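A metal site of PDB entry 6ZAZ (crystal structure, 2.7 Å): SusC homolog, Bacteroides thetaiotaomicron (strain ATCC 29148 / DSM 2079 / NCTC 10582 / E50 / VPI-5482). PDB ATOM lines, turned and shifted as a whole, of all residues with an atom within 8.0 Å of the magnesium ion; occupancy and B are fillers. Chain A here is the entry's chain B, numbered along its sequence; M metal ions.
N of His 865 lies close to OD1 of Asp 862, 3.4 Å away.
The side-chain carboxylate (OD2) of Asp 873 lies close to the backbone NH (N) of Asp 870 (3.0 Å).
OD1 of Asp 873 sits close to N of Ile 863 (3.0 Å).
The side-chain amide nitrogen of Asn 866 sits close to the guanidinium group of Arg 872.
N of Gly 867 lies within hydrogen-bond range of OD2 of Asp 862.
Of the 17 residues printed, 5 come within 4 Å of the magnesium ion.
Along chain A the residues within 4 Å of the magnesium ion span positions 862 to 873.
The nearest printed residue that does not touch the magnesium ion is His 865 (4.4 Å).
The magnesium ion is bound by the side-chain carboxylate (OD2) of Asp 864 (1.9 Å), the side-chain amide oxygen (OD1) of Asn 866 (2.1 Å), the side-chain carboxylate (OD1) of Asp 862 (2.3 Å), the backbone carbonyl oxygen (O) of Val 868 (2.4 Å), the side-chain carboxylate (OD2) of Asp 873 (2.4 Å) and the side-chain carboxylate (OD1) of Asp 873 (2.4 Å).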
ATOM      1  N   ALA A 848      11.927  23.068  18.422  1.00  0.00           N
ATOM      2  CA  ALA A 848      11.897  21.710  18.937  1.00  0.00           C
ATOM      3  C   ALA A 848      10.937  21.601  20.122  1.00  0.00           C
ATOM      4  O   ALA A 848      10.650  22.600  20.792  1.00  0.00           O
ATOM      5  CB  ALA A 848      13.296  21.241  19.340  1.00  0.00           C
ATOM      6  N   THR A 849      10.420  20.392  20.346  1.00  0.00           N
ATOM      7  CA  THR A 849       9.611  20.121  21.520  1.00  0.00           C
ATOM      8  C   THR A 849      10.412  20.420  22.774  1.00  0.00           C
ATOM      9  O   THR A 849      11.466  19.817  22.993  1.00  0.00           O
ATOM     10  CB  THR A 849       9.134  18.668  21.505  1.00  0.00           C
ATOM     11  OG1 THR A 849       8.101  18.530  20.530  1.00  0.00           O
ATOM     12  CG2 THR A 849       8.585  18.250  22.857  1.00  0.00           C
ATOM     13  N   TYR A 860      15.705  27.172  24.398  1.00  0.00           N
ATOM     14  CA  TYR A 860      16.962  26.445  24.506  1.00  0.00           C
ATOM     15  C   TYR A 860      17.275  25.723  23.188  1.00  0.00           C
ATOM     16  O   TYR A 860      16.393  25.131  22.551  1.00  0.00           O
ATOM     17  CB  TYR A 860      16.917  25.473  25.682  1.00  0.00           C
ATOM     18  CG  TYR A 860      17.047  26.153  27.041  1.00  0.00           C
ATOM     19  CD1 TYR A 860      18.238  26.801  27.397  1.00  0.00           C
ATOM     20  CD2 TYR A 860      15.989  26.157  27.957  1.00  0.00           C
ATOM     21  CE1 TYR A 860      18.366  27.431  28.635  1.00  0.00           C
ATOM     22  CE2 TYR A 860      16.107  26.794  29.224  1.00  0.00           C
ATOM     23  CZ  TYR A 860      17.306  27.422  29.557  1.00  0.00           C
ATOM     24  OH  TYR A 860      17.454  28.038  30.792  1.00  0.00           O
ATOM     25  N   ARG A 861      18.536  25.790  22.766  1.00  0.00           N
ATOM     26  CA  ARG A 861      18.946  25.329  21.451  1.00  0.00           C
ATOM     27  C   ARG A 861      18.884  23.817  21.327  1.00  0.00           C
ATOM     28  O   ARG A 861      19.219  23.081  22.261  1.00  0.00           O
ATOM     29  CB  ARG A 861      20.362  25.803  21.126  1.00  0.00           C
ATOM     30  CG  ARG A 861      20.823  25.387  19.720  1.00  0.00           C
ATOM     31  CD  ARG A 861      22.204  25.939  19.412  1.00  0.00           C
ATOM     32  NE  ARG A 861      22.280  27.383  19.567  1.00  0.00           N
ATOM     33  CZ  ARG A 861      23.385  28.085  19.397  1.00  0.00           C
ATOM     34  NH1 ARG A 861      24.519  27.461  19.072  1.00  0.00           N
ATOM     35  NH2 ARG A 861      23.389  29.403  19.568  1.00  0.00           N
ATOM     36  N   ASP A 862      18.498  23.356  20.131  1.00  0.00           N
ATOM     37  CA  ASP A 862      18.388  21.935  19.809  1.00  0.00           C
ATOM     38  C   ASP A 862      19.690  21.499  19.165  1.00  0.00           C
ATOM     39  O   ASP A 862      19.844  21.501  17.937  1.00  0.00           O
ATOM     40  CB  ASP A 862      17.180  21.714  18.897  1.00  0.00           C
ATOM     41  CG  ASP A 862      16.929  20.260  18.609  1.00  0.00           C
ATOM     42  OD1 ASP A 862      17.506  19.401  19.324  1.00  0.00           O
ATOM     43  OD2 ASP A 862      16.165  19.976  17.670  1.00  0.00           O
ATOM     44  N   ILE A 863      20.651  21.109  20.005  1.00  0.00           N
ATOM     45  CA  ILE A 863      22.035  20.971  19.533  1.00  0.00           C
ATOM     46  C   ILE A 863      22.187  19.745  18.644  1.00  0.00           C
ATOM     47  O   ILE A 863      22.916  19.780  17.645  1.00  0.00           O
ATOM     48  CB  ILE A 863      23.012  20.921  20.719  1.00  0.00           C
ATOM     49  CG1 ILE A 863      22.727  22.045  21.706  1.00  0.00           C
ATOM     50  CG2 ILE A 863      24.448  20.980  20.241  1.00  0.00           C
ATOM     51  CD1 ILE A 863      23.927  22.364  22.584  1.00  0.00           C
ATOM     52  N   ASP A 864      21.519  18.639  18.994  1.00  0.00           N
ATOM     53  CA  ASP A 864      21.583  17.396  18.224  1.00  0.00           C
ATOM     54  C   ASP A 864      20.599  17.372  17.060  1.00  0.00           C
ATOM     55  O   ASP A 864      20.650  16.437  16.251  1.00  0.00           O
ATOM     56  CB  ASP A 864      21.350  16.188  19.136  1.00  0.00           C
ATOM     57  CG  ASP A 864      20.141  16.343  20.014  1.00  0.00           C
ATOM     58  OD1 ASP A 864      20.031  15.578  20.982  1.00  0.00           O
ATOM     59  OD2 ASP A 864      19.335  17.262  19.766  1.00  0.00           O
ATOM     60  N   HIS A 865      19.710  18.359  16.983  1.00  0.00           N
ATOM     61  CA  HIS A 865      18.750  18.520  15.882  1.00  0.00           C
ATOM     62  C   HIS A 865      17.713  17.406  15.836  1.00  0.00           C
ATOM     63  O   HIS A 865      17.173  17.096  14.789  1.00  0.00           O
ATOM     64  CB  HIS A 865      19.483  18.639  14.549  1.00  0.00           C
ATOM     65  CG  HIS A 865      20.392  19.820  14.464  1.00  0.00           C
ATOM     66  ND1 HIS A 865      21.764  19.717  14.623  1.00  0.00           N
ATOM     67  CD2 HIS A 865      20.153  21.133  14.218  1.00  0.00           C
ATOM     68  CE1 HIS A 865      22.322  20.904  14.479  1.00  0.00           C
ATOM     69  NE2 HIS A 865      21.359  21.789  14.231  1.00  0.00           N
ATOM     70  N   ASN A 866      17.397  16.806  16.974  1.00  0.00           N
ATOM     71  CA  ASN A 866      16.501  15.663  17.010  1.00  0.00           C
ATOM     72  C   ASN A 866      15.035  16.060  17.161  1.00  0.00           C
ATOM     73  O   ASN A 866      14.189  15.169  17.299  1.00  0.00           O
ATOM     74  CB  ASN A 866      16.923  14.718  18.144  1.00  0.00           C
ATOM     75  CG  ASN A 866      16.885  15.403  19.517  1.00  0.00           C
ATOM     76  OD1 ASN A 866      16.497  16.568  19.641  1.00  0.00           O
ATOM     77  ND2 ASN A 866      17.285  14.668  20.544  1.00  0.00           N
ATOM     78  N   GLY A 867      14.727  17.360  17.145  1.00  0.00           N
ATOM     79  CA  GLY A 867      13.363  17.837  17.281  1.00  0.00           C
ATOM     80  C   GLY A 867      12.800  17.813  18.687  1.00  0.00           C
ATOM     81  O   GLY A 867      11.603  18.101  18.869  1.00  0.00           O
ATOM     82  N   VAL A 868      13.607  17.448  19.688  1.00  0.00           N
ATOM     83  CA  VAL A 868      13.222  17.504  21.098  1.00  0.00           C
ATOM     84  C   VAL A 868      14.318  18.244  21.844  1.00  0.00           C
ATOM     85  O   VAL A 868      15.510  18.038  21.592  1.00  0.00           O
ATOM     86  CB  VAL A 868      13.009  16.082  21.700  1.00  0.00           C
ATOM     87  CG1 VAL A 868      12.542  16.184  23.159  1.00  0.00           C
ATOM     88  CG2 VAL A 868      12.018  15.287  20.879  1.00  0.00           C
ATOM     89  N   ILE A 869      13.908  19.131  22.760  1.00  0.00           N
ATOM     90  CA  ILE A 869      14.834  19.760  23.693  1.00  0.00           C
ATOM     91  C   ILE A 869      14.867  18.940  24.974  1.00  0.00           C
ATOM     92  O   ILE A 869      13.907  18.957  25.751  1.00  0.00           O
ATOM     93  CB  ILE A 869      14.461  21.213  23.986  1.00  0.00           C
ATOM     94  CG1 ILE A 869      14.639  22.011  22.724  1.00  0.00           C
ATOM     95  CG2 ILE A 869      15.388  21.737  25.076  1.00  0.00           C
ATOM     96  CD1 ILE A 869      16.045  22.020  22.299  1.00  0.00           C
ATOM     97  N   ASP A 870      15.965  18.224  25.171  1.00  0.00           N
ATOM     98  CA  ASP A 870      16.091  17.301  26.277  1.00  0.00           C
ATOM     99  C   ASP A 870      17.547  17.324  26.740  1.00  0.00           C
ATOM    100  O   ASP A 870      18.362  18.105  26.253  1.00  0.00           O
ATOM    101  CB  ASP A 870      15.554  15.907  25.889  1.00  0.00           C
ATOM    102  CG  ASP A 870      16.603  14.984  25.239  1.00  0.00           C
ATOM    103  OD1 ASP A 870      17.705  15.428  24.809  1.00  0.00           O
ATOM    104  OD2 ASP A 870      16.282  13.772  25.154  1.00  0.00           O
ATOM    105  N   GLU A 871      17.862  16.440  27.705  1.00  0.00           N
ATOM    106  CA  GLU A 871      19.108  16.534  28.446  1.00  0.00           C
ATOM    107  C   GLU A 871      20.335  16.353  27.570  1.00  0.00           C
ATOM    108  O   GLU A 871      21.438  16.613  28.058  1.00  0.00           O
ATOM    109  CB  GLU A 871      19.105  15.501  29.577  1.00  0.00           C
ATOM    110  CG  GLU A 871      19.816  14.213  29.276  1.00  0.00           C
ATOM    111  CD  GLU A 871      19.548  13.178  30.338  1.00  0.00           C
ATOM    112  OE1 GLU A 871      18.441  13.197  30.913  1.00  0.00           O
ATOM    113  OE2 GLU A 871      20.435  12.345  30.610  1.00  0.00           O
ATOM    114  N   ARG A 872      20.182  15.926  26.317  1.00  0.00           N
ATOM    115  CA  ARG A 872      21.297  15.720  25.397  1.00  0.00           C
ATOM    116  C   ARG A 872      21.793  17.010  24.761  1.00  0.00           C
ATOM    117  O   ARG A 872      22.883  17.018  24.184  1.00  0.00           O
ATOM    118  CB  ARG A 872      20.880  14.740  24.309  1.00  0.00           C
ATOM    119  CG  ARG A 872      20.893  13.292  24.747  1.00  0.00           C
ATOM    120  CD  ARG A 872      20.391  12.406  23.652  1.00  0.00           C
ATOM    121  NE  ARG A 872      18.948  12.539  23.472  1.00  0.00           N
ATOM    122  CZ  ARG A 872      18.260  11.895  22.537  1.00  0.00           C
ATOM    123  NH1 ARG A 872      18.872  11.067  21.680  1.00  0.00           N
ATOM    124  NH2 ARG A 872      16.951  12.078  22.469  1.00  0.00           N
ATOM    125  N   ASP A 873      21.024  18.090  24.874  1.00  0.00           N
ATOM    126  CA  ASP A 873      21.315  19.321  24.156  1.00  0.00           C
ATOM    127  C   ASP A 873      22.154  20.279  24.988  1.00  0.00           C
ATOM    128  O   ASP A 873      21.797  21.437  25.184  1.00  0.00           O
ATOM    129  CB  ASP A 873      19.996  19.958  23.730  1.00  0.00           C
ATOM    130  CG  ASP A 873      19.210  19.097  22.750  1.00  0.00           C
ATOM    131  OD1 ASP A 873      19.775  18.789  21.690  1.00  0.00           O
ATOM    132  OD2 ASP A 873      18.054  18.714  23.037  1.00  0.00           O
ATOM    133  N   GLN A 874      23.276  19.792  25.514  1.00  0.00           N
ATOM    134  CA  GLN A 874      24.205  20.627  26.267  1.00  0.00           C
ATOM    135  C   GLN A 874      25.600  20.530  25.678  1.00  0.00           C
ATOM    136  O   GLN A 874      25.969  19.557  25.017  1.00  0.00           O
ATOM    137  CB  GLN A 874      24.263  20.237  27.744  1.00  0.00           C
ATOM    138  CG  GLN A 874      22.929  19.876  28.378  1.00  0.00           C
ATOM    139  CD  GLN A 874      23.092  19.600  29.847  1.00  0.00           C
ATOM    140  OE1 GLN A 874      23.921  20.243  30.500  1.00  0.00           O
ATOM    141  NE2 GLN A 874      22.317  18.661  30.387  1.00  0.00           N
HETATM  142 MG    MG M   1      17.777  17.648  20.858  1.00  0.00          MG
